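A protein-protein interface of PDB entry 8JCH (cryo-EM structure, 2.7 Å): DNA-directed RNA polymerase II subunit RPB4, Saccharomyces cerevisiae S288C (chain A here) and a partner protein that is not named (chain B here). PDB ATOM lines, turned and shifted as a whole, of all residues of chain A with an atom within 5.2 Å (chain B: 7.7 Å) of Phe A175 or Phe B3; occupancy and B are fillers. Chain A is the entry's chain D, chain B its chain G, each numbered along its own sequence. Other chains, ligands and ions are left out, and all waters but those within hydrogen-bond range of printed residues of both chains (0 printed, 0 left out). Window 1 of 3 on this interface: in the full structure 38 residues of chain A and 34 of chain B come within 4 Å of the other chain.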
ATOM      1  N   LEU A  29     -18.647  -2.443 -30.630  1.00  0.00           N
ATOM      2  CA  LEU A  29     -18.135  -2.172 -29.298  1.00  0.00           C
ATOM      3  C   LEU A  29     -17.337  -3.369 -28.780  1.00  0.00           C
ATOM      4  O   LEU A  29     -17.395  -4.476 -29.323  1.00  0.00           O
ATOM      5  CB  LEU A  29     -19.278  -1.842 -28.339  1.00  0.00           C
ATOM      6  CG  LEU A  29     -20.223  -0.701 -28.727  1.00  0.00           C
ATOM      7  CD1 LEU A  29     -21.447  -1.231 -29.461  1.00  0.00           C
ATOM      8  CD2 LEU A  29     -20.640   0.091 -27.497  1.00  0.00           C
ATOM      9  N   PHE A  33     -18.003  -4.355 -23.100  1.00  0.00           N
ATOM     10  CA  PHE A  33     -19.133  -3.441 -23.269  1.00  0.00           C
ATOM     11  C   PHE A  33     -19.989  -3.898 -24.450  1.00  0.00           C
ATOM     12  O   PHE A  33     -20.003  -3.300 -25.526  1.00  0.00           O
ATOM     13  CB  PHE A  33     -18.639  -2.009 -23.451  1.00  0.00           C
ATOM     14  CG  PHE A  33     -17.613  -1.588 -22.441  1.00  0.00           C
ATOM     15  CD1 PHE A  33     -17.987  -1.286 -21.142  1.00  0.00           C
ATOM     16  CD2 PHE A  33     -16.278  -1.483 -22.790  1.00  0.00           C
ATOM     17  CE1 PHE A  33     -17.048  -0.895 -20.209  1.00  0.00           C
ATOM     18  CE2 PHE A  33     -15.335  -1.092 -21.860  1.00  0.00           C
ATOM     19  CZ  PHE A  33     -15.719  -0.798 -20.569  1.00  0.00           C
ATOM     20  N   LEU A  47     -26.876  -2.738 -21.727  1.00  0.00           N
ATOM     21  CA  LEU A  47     -25.838  -1.855 -21.215  1.00  0.00           C
ATOM     22  C   LEU A  47     -26.410  -0.477 -20.905  1.00  0.00           C
ATOM     23  O   LEU A  47     -27.221   0.063 -21.662  1.00  0.00           O
ATOM     24  CB  LEU A  47     -24.699  -1.735 -22.228  1.00  0.00           C
ATOM     25  CG  LEU A  47     -23.554  -0.787 -21.865  1.00  0.00           C
ATOM     26  CD1 LEU A  47     -22.884  -1.224 -20.571  1.00  0.00           C
ATOM     27  CD2 LEU A  47     -22.542  -0.704 -22.997  1.00  0.00           C
ATOM     28  N   ILE A  48     -25.982   0.090 -19.782  1.00  0.00           N
ATOM     29  CA  ILE A  48     -26.427   1.412 -19.356  1.00  0.00           C
ATOM     30  C   ILE A  48     -25.451   2.453 -19.888  1.00  0.00           C
ATOM     31  O   ILE A  48     -24.240   2.360 -19.658  1.00  0.00           O
ATOM     32  CB  ILE A  48     -26.540   1.496 -17.823  1.00  0.00           C
ATOM     33  CG1 ILE A  48     -27.478   0.422 -17.248  1.00  0.00           C
ATOM     34  CG2 ILE A  48     -27.006   2.883 -17.400  1.00  0.00           C
ATOM     35  CD1 ILE A  48     -28.589  -0.053 -18.175  1.00  0.00           C
ATOM     36  N   ALA A  49     -25.979   3.445 -20.599  1.00  0.00           N
ATOM     37  CA  ALA A  49     -25.186   4.533 -21.154  1.00  0.00           C
ATOM     38  C   ALA A  49     -25.560   5.831 -20.453  1.00  0.00           C
ATOM     39  O   ALA A  49     -26.747   6.149 -20.318  1.00  0.00           O
ATOM     40  CB  ALA A  49     -25.405   4.659 -22.662  1.00  0.00           C
ATOM     41  N   LEU A  50     -24.550   6.575 -20.011  1.00  0.00           N
ATOM     42  CA  LEU A  50     -24.746   7.812 -19.270  1.00  0.00           C
ATOM     43  C   LEU A  50     -24.232   8.988 -20.087  1.00  0.00           C
ATOM     44  O   LEU A  50     -23.141   8.920 -20.664  1.00  0.00           O
ATOM     45  CB  LEU A  50     -24.030   7.760 -17.918  1.00  0.00           C
ATOM     46  CG  LEU A  50     -24.656   6.860 -16.853  1.00  0.00           C
ATOM     47  CD1 LEU A  50     -23.953   5.514 -16.810  1.00  0.00           C
ATOM     48  CD2 LEU A  50     -24.613   7.534 -15.492  1.00  0.00           C
ATOM     49  N   HIS A 173     -29.570   2.695 -30.222  1.00  0.00           N
ATOM     50  CA  HIS A 173     -28.650   2.140 -29.239  1.00  0.00           C
ATOM     51  C   HIS A 173     -28.313   3.230 -28.226  1.00  0.00           C
ATOM     52  O   HIS A 173     -28.017   4.363 -28.622  1.00  0.00           O
ATOM     53  CB  HIS A 173     -27.400   1.613 -29.966  1.00  0.00           C
ATOM     54  CG  HIS A 173     -26.322   1.069 -29.074  1.00  0.00           C
ATOM     55  ND1 HIS A 173     -25.979   1.627 -27.862  1.00  0.00           N
ATOM     56  CD2 HIS A 173     -25.504   0.001 -29.235  1.00  0.00           C
ATOM     57  CE1 HIS A 173     -25.002   0.927 -27.313  1.00  0.00           C
ATOM     58  NE2 HIS A 173     -24.694  -0.064 -28.128  1.00  0.00           N
ATOM     59  N   PRO A 174     -28.362   2.940 -26.922  1.00  0.00           N
ATOM     60  CA  PRO A 174     -28.197   4.008 -25.920  1.00  0.00           C
ATOM     61  C   PRO A 174     -26.884   4.768 -26.022  1.00  0.00           C
ATOM     62  O   PRO A 174     -26.789   5.879 -25.485  1.00  0.00           O
ATOM     63  CB  PRO A 174     -28.297   3.256 -24.587  1.00  0.00           C
ATOM     64  CG  PRO A 174     -29.111   2.050 -24.897  1.00  0.00           C
ATOM     65  CD  PRO A 174     -28.782   1.666 -26.313  1.00  0.00           C
ATOM     66  N   PHE A 175     -25.868   4.207 -26.679  1.00  0.00           N
ATOM     67  CA  PHE A 175     -24.596   4.909 -26.812  1.00  0.00           C
ATOM     68  C   PHE A 175     -24.737   6.148 -27.691  1.00  0.00           C
ATOM     69  O   PHE A 175     -24.280   7.236 -27.322  1.00  0.00           O
ATOM     70  CB  PHE A 175     -23.537   3.961 -27.375  1.00  0.00           C
ATOM     71  CG  PHE A 175     -22.173   4.575 -27.491  1.00  0.00           C
ATOM     72  CD1 PHE A 175     -21.774   5.198 -28.661  1.00  0.00           C
ATOM     73  CD2 PHE A 175     -21.293   4.534 -26.424  1.00  0.00           C
ATOM     74  CE1 PHE A 175     -20.521   5.762 -28.763  1.00  0.00           C
ATOM     75  CE2 PHE A 175     -20.039   5.097 -26.522  1.00  0.00           C
ATOM     76  CZ  PHE A 175     -19.652   5.712 -27.693  1.00  0.00           C
ATOM     77  N   GLU A 176     -25.369   6.003 -28.859  1.00  0.00           N
ATOM     78  CA  GLU A 176     -25.493   7.139 -29.767  1.00  0.00           C
ATOM     79  C   GLU A 176     -26.459   8.188 -29.231  1.00  0.00           C
ATOM     80  O   GLU A 176     -26.260   9.387 -29.467  1.00  0.00           O
ATOM     81  CB  GLU A 176     -25.924   6.666 -31.156  1.00  0.00           C
ATOM     82  CG  GLU A 176     -27.277   5.978 -31.209  1.00  0.00           C
ATOM     83  CD  GLU A 176     -27.276   4.762 -32.115  1.00  0.00           C
ATOM     84  OE1 GLU A 176     -26.287   4.572 -32.853  1.00  0.00           O
ATOM     85  OE2 GLU A 176     -28.263   3.999 -32.090  1.00  0.00           O
ATOM     86  N   VAL A 177     -27.503   7.768 -28.512  1.00  0.00           N
ATOM     87  CA  VAL A 177     -28.394   8.744 -27.895  1.00  0.00           C
ATOM     88  C   VAL A 177     -27.649   9.528 -26.820  1.00  0.00           C
ATOM     89  O   VAL A 177     -27.857  10.737 -26.659  1.00  0.00           O
ATOM     90  CB  VAL A 177     -29.668   8.060 -27.354  1.00  0.00           C
ATOM     91  CG1 VAL A 177     -30.088   6.922 -28.274  1.00  0.00           C
ATOM     92  CG2 VAL A 177     -29.490   7.560 -25.926  1.00  0.00           C
ATOM     93  N   ALA A 178     -26.734   8.869 -26.102  1.00  0.00           N
ATOM     94  CA  ALA A 178     -25.890   9.582 -25.151  1.00  0.00           C
ATOM     95  C   ALA A 178     -24.964  10.558 -25.865  1.00  0.00           C
ATOM     96  O   ALA A 178     -24.733  11.672 -25.381  1.00  0.00           O
ATOM     97  CB  ALA A 178     -25.084   8.589 -24.315  1.00  0.00           C
ATOM     98  N   GLN A 179     -24.426  10.155 -27.019  1.00  0.00           N
ATOM     99  CA  GLN A 179     -23.547  11.040 -27.775  1.00  0.00           C
ATOM    100  C   GLN A 179     -24.286  12.284 -28.252  1.00  0.00           C
ATOM    101  O   GLN A 179     -23.754  13.397 -28.171  1.00  0.00           O
ATOM    102  CB  GLN A 179     -22.938  10.290 -28.960  1.00  0.00           C
ATOM    103  CG  GLN A 179     -21.932   9.226 -28.563  1.00  0.00           C
ATOM    104  CD  GLN A 179     -20.533   9.788 -28.394  1.00  0.00           C
ATOM    105  OE1 GLN A 179     -20.317  10.993 -28.517  1.00  0.00           O
ATOM    106  NE2 GLN A 179     -19.575   8.914 -28.108  1.00  0.00           N
ATOM    107  N   MET B   1     -21.086   8.219 -22.984  1.00  0.00           N
ATOM    108  CA  MET B   1     -19.809   7.523 -23.062  1.00  0.00           C
ATOM    109  C   MET B   1     -19.573   6.845 -21.716  1.00  0.00           C
ATOM    110  O   MET B   1     -19.044   5.737 -21.651  1.00  0.00           O
ATOM    111  CB  MET B   1     -18.690   8.513 -23.455  1.00  0.00           C
ATOM    112  CG  MET B   1     -17.207   8.065 -23.393  1.00  0.00           C
ATOM    113  SD  MET B   1     -16.461   7.297 -21.936  1.00  0.00           S
ATOM    114  CE  MET B   1     -16.839   8.508 -20.672  1.00  0.00           C
ATOM    115  N   PHE B   2     -19.999   7.510 -20.644  1.00  0.00           N
ATOM    116  CA  PHE B   2     -19.861   6.949 -19.307  1.00  0.00           C
ATOM    117  C   PHE B   2     -20.750   5.721 -19.152  1.00  0.00           C
ATOM    118  O   PHE B   2     -21.940   5.757 -19.478  1.00  0.00           O
ATOM    119  CB  PHE B   2     -20.225   7.996 -18.256  1.00  0.00           C
ATOM    120  CG  PHE B   2     -19.183   9.060 -18.073  1.00  0.00           C
ATOM    121  CD1 PHE B   2     -18.136   8.876 -17.185  1.00  0.00           C
ATOM    122  CD2 PHE B   2     -19.252  10.246 -18.783  1.00  0.00           C
ATOM    123  CE1 PHE B   2     -17.177   9.854 -17.012  1.00  0.00           C
ATOM    124  CE2 PHE B   2     -18.294  11.228 -18.615  1.00  0.00           C
ATOM    125  CZ  PHE B   2     -17.256  11.031 -17.728  1.00  0.00           C
ATOM    126  N   PHE B   3     -20.170   4.636 -18.648  1.00  0.00           N
ATOM    127  CA  PHE B   3     -20.890   3.397 -18.396  1.00  0.00           C
ATOM    128  C   PHE B   3     -20.707   2.976 -16.944  1.00  0.00           C
ATOM    129  O   PHE B   3     -19.741   3.358 -16.278  1.00  0.00           O
ATOM    130  CB  PHE B   3     -20.417   2.262 -19.317  1.00  0.00           C
ATOM    131  CG  PHE B   3     -20.308   2.650 -20.765  1.00  0.00           C
ATOM    132  CD1 PHE B   3     -21.309   3.381 -21.382  1.00  0.00           C
ATOM    133  CD2 PHE B   3     -19.203   2.276 -21.510  1.00  0.00           C
ATOM    134  CE1 PHE B   3     -21.208   3.734 -22.714  1.00  0.00           C
ATOM    135  CE2 PHE B   3     -19.095   2.626 -22.841  1.00  0.00           C
ATOM    136  CZ  PHE B   3     -20.099   3.355 -23.444  1.00  0.00           C
ATOM    137  N   ILE B   4     -21.657   2.182 -16.460  1.00  0.00           N
ATOM    138  CA  ILE B   4     -21.575   1.549 -15.149  1.00  0.00           C
ATOM    139  C   ILE B   4     -21.707   0.049 -15.360  1.00  0.00           C
ATOM    140  O   ILE B   4     -22.684  -0.416 -15.960  1.00  0.00           O
ATOM    141  CB  ILE B   4     -22.652   2.073 -14.187  1.00  0.00           C
ATOM    142  CG1 ILE B   4     -23.956   2.341 -14.937  1.00  0.00           C
ATOM    143  CG2 ILE B   4     -22.171   3.333 -13.486  1.00  0.00           C
ATOM    144  CD1 ILE B   4     -25.103   2.746 -14.040  1.00  0.00           C
ATOM    145  N   LYS B   5     -20.727  -0.708 -14.872  1.00  0.00           N
ATOM    146  CA  LYS B   5     -20.685  -2.147 -15.072  1.00  0.00           C
ATOM    147  C   LYS B   5     -20.525  -2.850 -13.734  1.00  0.00           C
ATOM    148  O   LYS B   5     -19.937  -2.309 -12.793  1.00  0.00           O
ATOM    149  CB  LYS B   5     -19.543  -2.549 -16.014  1.00  0.00           C
ATOM    150  CG  LYS B   5     -19.900  -2.477 -17.489  1.00  0.00           C
ATOM    151  CD  LYS B   5     -19.176  -3.551 -18.285  1.00  0.00           C
ATOM    152  CE  LYS B   5     -19.385  -4.928 -17.678  1.00  0.00           C
ATOM    153  NZ  LYS B   5     -20.830  -5.268 -17.552  1.00  0.00           N
ATOM    154  N   LEU B   7     -18.610  -4.879 -12.049  1.00  0.00           N
ATOM    155  CA  LEU B   7     -17.268  -5.435 -11.995  1.00  0.00           C
ATOM    156  C   LEU B   7     -17.136  -6.396 -10.815  1.00  0.00           C
ATOM    157  O   LEU B   7     -17.968  -6.432  -9.904  1.00  0.00           O
ATOM    158  CB  LEU B   7     -16.232  -4.319 -11.888  1.00  0.00           C
ATOM    159  CG  LEU B   7     -15.641  -3.756 -13.181  1.00  0.00           C
ATOM    160  CD1 LEU B   7     -16.635  -2.837 -13.867  1.00  0.00           C
ATOM    161  CD2 LEU B   7     -14.346  -3.020 -12.888  1.00  0.00           C
ATOM    162  N   PHE B  42     -11.280  -2.662 -18.548  1.00  0.00           N
ATOM    163  CA  PHE B  42     -12.432  -1.821 -18.244  1.00  0.00           C
ATOM    164  C   PHE B  42     -12.161  -0.362 -18.590  1.00  0.00           C
ATOM    165  O   PHE B  42     -13.027   0.319 -19.151  1.00  0.00           O
ATOM    166  CB  PHE B  42     -12.808  -1.964 -16.770  1.00  0.00           C
ATOM    167  CG  PHE B  42     -13.134  -3.372 -16.364  1.00  0.00           C
ATOM    168  CD1 PHE B  42     -14.309  -3.974 -16.781  1.00  0.00           C
ATOM    169  CD2 PHE B  42     -12.261  -4.096 -15.569  1.00  0.00           C
ATOM    170  CE1 PHE B  42     -14.610  -5.270 -16.410  1.00  0.00           C
ATOM    171  CE2 PHE B  42     -12.557  -5.393 -15.193  1.00  0.00           C
ATOM    172  CZ  PHE B  42     -13.733  -5.980 -15.615  1.00  0.00           C
ATOM    173  N   TYR B  44     -10.891   3.462 -17.132  1.00  0.00           N
ATOM    174  CA  TYR B  44     -10.661   4.320 -15.978  1.00  0.00           C
ATOM    175  C   TYR B  44     -11.826   4.191 -15.007  1.00  0.00           C
ATOM    176  O   TYR B  44     -12.986   4.365 -15.393  1.00  0.00           O
ATOM    177  CB  TYR B  44     -10.498   5.780 -16.406  1.00  0.00           C
ATOM    178  CG  TYR B  44      -9.090   6.167 -16.791  1.00  0.00           C
ATOM    179  CD1 TYR B  44      -8.073   6.192 -15.846  1.00  0.00           C
ATOM    180  CD2 TYR B  44      -8.777   6.512 -18.099  1.00  0.00           C
ATOM    181  CE1 TYR B  44      -6.786   6.550 -16.192  1.00  0.00           C
ATOM    182  CE2 TYR B  44      -7.491   6.868 -18.456  1.00  0.00           C
ATOM    183  CZ  TYR B  44      -6.500   6.885 -17.498  1.00  0.00           C
ATOM    184  OH  TYR B  44      -5.217   7.241 -17.849  1.00  0.00           O
ATOM    185  N   ILE B  45     -11.515   3.892 -13.749  1.00  0.00           N
ATOM    186  CA  ILE B  45     -12.511   3.814 -12.688  1.00  0.00           C
ATOM    187  C   ILE B  45     -12.448   5.112 -11.897  1.00  0.00           C
ATOM    188  O   ILE B  45     -11.399   5.462 -11.343  1.00  0.00           O
ATOM    189  CB  ILE B  45     -12.273   2.598 -11.780  1.00  0.00           C
ATOM    190  CG1 ILE B  45     -11.990   1.351 -12.621  1.00  0.00           C
ATOM    191  CG2 ILE B  45     -13.474   2.369 -10.877  1.00  0.00           C
ATOM    192  CD1 ILE B  45     -13.167   0.900 -13.456  1.00  0.00           C
ATOM    193  N   CYS B  47     -15.501   6.622  -9.772  1.00  0.00           N
ATOM    194  CA  CYS B  47     -16.249   6.599  -8.525  1.00  0.00           C
ATOM    195  C   CYS B  47     -16.880   5.231  -8.325  1.00  0.00           C
ATOM    196  O   CYS B  47     -17.257   4.554  -9.285  1.00  0.00           O
ATOM    197  CB  CYS B  47     -17.337   7.681  -8.502  1.00  0.00           C
ATOM    198  SG  CYS B  47     -18.794   7.249  -7.524  1.00  0.00           S
ATOM    199  N   LEU B  49     -20.019   3.835  -6.851  1.00  0.00           N
ATOM    200  CA  LEU B  49     -21.355   4.102  -6.347  1.00  0.00           C
ATOM    201  C   LEU B  49     -21.942   2.852  -5.695  1.00  0.00           C
ATOM    202  O   LEU B  49     -21.355   1.768  -5.720  1.00  0.00           O
ATOM    203  CB  LEU B  49     -22.262   4.598  -7.474  1.00  0.00           C
ATOM    204  CG  LEU B  49     -22.976   3.555  -8.338  1.00  0.00           C
ATOM    205  CD1 LEU B  49     -24.097   4.204  -9.134  1.00  0.00           C
ATOM    206  CD2 LEU B  49     -22.000   2.853  -9.269  1.00  0.00           C
ATOM    207  N   ARG B  75     -20.383  -2.234  -8.328  1.00  0.00           N
ATOM    208  CA  ARG B  75     -20.602  -1.494  -9.562  1.00  0.00           C
ATOM    209  C   ARG B  75     -19.924  -0.137  -9.453  1.00  0.00           C
ATOM    210  O   ARG B  75     -19.914   0.476  -8.382  1.00  0.00           O
ATOM    211  CB  ARG B  75     -22.096  -1.316  -9.849  1.00  0.00           C
ATOM    212  CG  ARG B  75     -22.948  -1.167  -8.601  1.00  0.00           C
ATOM    213  CD  ARG B  75     -24.407  -1.480  -8.887  1.00  0.00           C
ATOM    214  NE  ARG B  75     -24.949  -0.640  -9.947  1.00  0.00           N
ATOM    215  CZ  ARG B  75     -25.407  -1.096 -11.103  1.00  0.00           C
ATOM    216  NH1 ARG B  75     -25.402  -2.389 -11.388  1.00  0.00           N
ATOM    217  NH2 ARG B  75     -25.884  -0.236 -11.999  1.00  0.00           N
ATOM    218  N   ALA B  76     -19.358   0.329 -10.565  1.00  0.00           N
ATOM    219  CA  ALA B  76     -18.634   1.591 -10.569  1.00  0.00           C
ATOM    220  C   ALA B  76     -18.714   2.217 -11.953  1.00  0.00           C
ATOM    221  O   ALA B  76     -18.995   1.543 -12.948  1.00  0.00           O
ATOM    222  CB  ALA B  76     -17.172   1.401 -10.151  1.00  0.00           C
ATOM    223  N   VAL B  77     -18.463   3.521 -12.001  1.00  0.00           N
ATOM    224  CA  VAL B  77     -18.450   4.258 -13.260  1.00  0.00           C
ATOM    225  C   VAL B  77     -17.118   4.023 -13.957  1.00  0.00           C
ATOM    226  O   VAL B  77     -16.052   4.159 -13.348  1.00  0.00           O
ATOM    227  CB  VAL B  77     -18.694   5.756 -13.016  1.00  0.00           C
ATOM    228  CG1 VAL B  77     -18.890   6.482 -14.336  1.00  0.00           C
ATOM    229  CG2 VAL B  77     -19.895   5.955 -12.106  1.00  0.00           C
ATOM    230  N   VAL B  78     -17.175   3.672 -15.239  1.00  0.00           N
ATOM    231  CA  VAL B  78     -15.982   3.370 -16.013  1.00  0.00           C
ATOM    232  C   VAL B  78     -15.774   4.455 -17.062  1.00  0.00           C
ATOM    233  O   VAL B  78     -16.673   5.236 -17.384  1.00  0.00           O
ATOM    234  CB  VAL B  78     -16.057   1.979 -16.674  1.00  0.00           C
ATOM    235  CG1 VAL B  78     -16.235   0.899 -15.618  1.00  0.00           C
ATOM    236  CG2 VAL B  78     -17.182   1.932 -17.692  1.00  0.00           C
ATOM    237  N   PHE B  79     -14.555   4.496 -17.599  1.00  0.00           N
ATOM    238  CA  PHE B  79     -14.181   5.478 -18.613  1.00  0.00           C
ATOM    239  C   PHE B  79     -13.191   4.809 -19.556  1.00  0.00           C
ATOM    240  O   PHE B  79     -12.086   4.447 -19.140  1.00  0.00           O
ATOM    241  CB  PHE B  79     -13.577   6.727 -17.970  1.00  0.00           C
ATOM    242  CG  PHE B  79     -13.639   7.960 -18.834  1.00  0.00           C
ATOM    243  CD1 PHE B  79     -13.300   7.912 -20.177  1.00  0.00           C
ATOM    244  CD2 PHE B  79     -14.026   9.175 -18.293  1.00  0.00           C
ATOM    245  CE1 PHE B  79     -13.352   9.048 -20.962  1.00  0.00           C
ATOM    246  CE2 PHE B  79     -14.082  10.313 -19.074  1.00  0.00           C
ATOM    247  CZ  PHE B  79     -13.744  10.249 -20.411  1.00  0.00           C
ATOM    248  N   LYS B  80     -13.585   4.646 -20.818  1.00  0.00           N
ATOM    249  CA  LYS B  80     -12.722   4.060 -21.832  1.00  0.00           C
ATOM    250  C   LYS B  80     -12.797   4.911 -23.096  1.00  0.00           C
ATOM    251  O   LYS B  80     -13.904   5.258 -23.544  1.00  0.00           O
ATOM    252  CB  LYS B  80     -13.124   2.610 -22.136  1.00  0.00           C
ATOM    253  CG  LYS B  80     -12.090   1.837 -22.942  1.00  0.00           C
ATOM    254  CD  LYS B  80     -12.358   0.344 -22.920  1.00  0.00           C
ATOM    255  CE  LYS B  80     -11.208  -0.431 -23.544  1.00  0.00           C
ATOM    256  NZ  LYS B  80      -9.952  -0.288 -22.759  1.00  0.00           N
ATOM    257  N   PHE B  82     -13.208   5.042 -26.466  1.00  0.00           N
ATOM    258  CA  PHE B  82     -13.596   4.257 -27.630  1.00  0.00           C
ATOM    259  C   PHE B  82     -13.097   4.913 -28.911  1.00  0.00           C
ATOM    260  O   PHE B  82     -13.229   6.127 -29.096  1.00  0.00           O
ATOM    261  CB  PHE B  82     -15.114   4.096 -27.670  1.00  0.00           C
ATOM    262  CG  PHE B  82     -15.592   2.743 -27.229  1.00  0.00           C
ATOM    263  CD1 PHE B  82     -16.765   2.209 -27.733  1.00  0.00           C
ATOM    264  CD2 PHE B  82     -14.866   2.007 -26.308  1.00  0.00           C
ATOM    265  CE1 PHE B  82     -17.205   0.964 -27.326  1.00  0.00           C
ATOM    266  CE2 PHE B  82     -15.302   0.761 -25.897  1.00  0.00           C
ATOM    267  CZ  PHE B  82     -16.473   0.239 -26.408  1.00  0.00           C
ATOM    268  N   LYS B  83     -12.520   4.103 -29.795  1.00  0.00           N
ATOM    269  CA  LYS B  83     -11.953   4.618 -31.035  1.00  0.00           C
ATOM    270  C   LYS B  83     -13.051   5.142 -31.953  1.00  0.00           C
ATOM    271  O   LYS B  83     -14.135   4.560 -32.050  1.00  0.00           O
ATOM    272  CB  LYS B  83     -11.143   3.525 -31.735  1.00  0.00           C
ATOM    273  CG  LYS B  83     -11.358   3.430 -33.238  1.00  0.00           C
ATOM    274  CD  LYS B  83     -10.409   2.425 -33.870  1.00  0.00           C
ATOM    275  CE  LYS B  83     -10.381   2.569 -35.383  1.00  0.00           C
ATOM    276  NZ  LYS B  83      -9.674   3.808 -35.809  1.00  0.00           N
ATOM    277  N   GLY B  84     -12.764   6.255 -32.626  1.00  0.00           N
ATOM    278  CA  GLY B  84     -13.725   6.846 -33.533  1.00  0.00           C
ATOM    279  C   GLY B  84     -14.815   7.652 -32.869  1.00  0.00           C
ATOM    280  O   GLY B  84     -15.828   7.947 -33.510  1.00  0.00           O
ATOM    281  N   GLU B  85     -14.643   8.019 -31.604  1.00  0.00           N
ATOM    282  CA  GLU B  85     -15.662   8.737 -30.853  1.00  0.00           C
ATOM    283  C   GLU B  85     -15.286  10.208 -30.743  1.00  0.00           C
ATOM    284  O   GLU B  85     -14.141  10.541 -30.421  1.00  0.00           O
ATOM    285  CB  GLU B  85     -15.837   8.131 -29.460  1.00  0.00           C
ATOM    286  CG  GLU B  85     -16.956   7.101 -29.358  1.00  0.00           C
ATOM    287  CD  GLU B  85     -18.051   7.289 -30.397  1.00  0.00           C
ATOM    288  OE1 GLU B  85     -18.671   8.374 -30.436  1.00  0.00           O
ATOM    289  OE2 GLU B  85     -18.293   6.346 -31.179  1.00  0.00           O
ATOM    290  N   VAL B  86     -16.251  11.080 -31.014  1.00  0.00           N
ATOM    291  CA  VAL B  86     -16.039  12.522 -30.960  1.00  0.00           C
ATOM    292  C   VAL B  86     -16.242  12.990 -29.524  1.00  0.00           C
ATOM    293  O   VAL B  86     -17.296  12.749 -28.926  1.00  0.00           O
ATOM    294  CB  VAL B  86     -16.986  13.257 -31.919  1.00  0.00           C
ATOM    295  CG1 VAL B  86     -17.026  14.740 -31.592  1.00  0.00           C
ATOM    296  CG2 VAL B  86     -16.555  13.036 -33.360  1.00  0.00           C
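NE2 of Gln A179 is in hydrogen-bond range of OE1 of Glu B85 (2.6 Å).
The backbone carbonyl oxygen (O) of Phe B2 is in hydrogen-bond range of the backbone NH (N) of Leu A50 (2.8 Å).
O of Leu A50 sits at hydrogen-bond distance from N of Met B1 (3.2 Å).
O of Phe B3 is in hydrogen-bond range of N of Val B78, at 2.8 Å.
The backbone carbonyl oxygen (O) of Ala B76 is in hydrogen-bond range of the backbone NH (N) of Lys B5 (3.4 Å).
A ring nitrogen (ND1) of His A173 lies within hydrogen-bond range of the backbone NH (N) of Phe A175.
Phe B82 touches Leu A29 (CE1 to CD2, 3.5 Å).
Phe B3 touches Phe A33 (CD2 to CD1, 3.8 Å).
Lys B5 touches Phe A33 (CD to CD1, 3.8 Å).
CZ of Phe A33 touches O of Phe B42 (3.2 Å).
CE1 of Phe A33 touches CG2 of Val B78, at 3.8 Å.
Phe A33 touches Phe B82 (CD2 to CE2, 3.95 Å).
Ile A48 touches Phe B3 (O to CD1, 3.6 Å).
Ile B4 touches Ile A48.
Ala A49 touches Phe B2 (C to O, 3.7 Å).
CZ of Phe B3 touches CD2 of Phe A175, 3.4 Å away.
Of chain B, only Phe B3 (3.4 Å) and Glu B85 (3.3 Å) come within 4 Å of Phe A175.
Of the printed residues of chain A, Phe B3 touches Phe A33 (3.8 Å), Ile A48 (3.6 Å) and Phe A175 (3.4 Å).
Printed residues of chain B within 4 Å of Ala A49: Phe B2 (3.7 Å).
Of the printed residues of chain B, Leu A50 touches Met B1, Phe B2 and Ile B4.
Of the printed residues of chain A, Phe B42 touches Phe A33.
Cys B47 touches none of the printed residues of chain A.
Ile B45 touches none of the printed residues of chain A.
The nearest residue of chain B that does not touch Phe A175 is Met B1 (4.2 Å).
The nearest printed residue of chain A that does not touch Phe B3 is Leu A50 (4.05 Å).
The nearest printed residue of chain A that does not touch Val B78 is Leu A47 (7.1 Å).
Of the 22 printed residues of chain B, 11 touch a printed residue of chain A.
Printed residues of chain B that touch a printed residue of chain A: Met B1, Phe B2, Phe B3, Ile B4, Lys B5, Phe B42, Val B78, Lys B80, Phe B82, Glu B85 and Val B86.
Hydrophobic or aromatic side chains of chain B that line the printed part of chain A: Phe B2, Phe B3, Ile B4, Val B78 and Phe B82.
Among the printed residues, no Asp or Glu carboxylate lies within 4 Å of a Lys or Arg side-chain nitrogen of the other chain.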
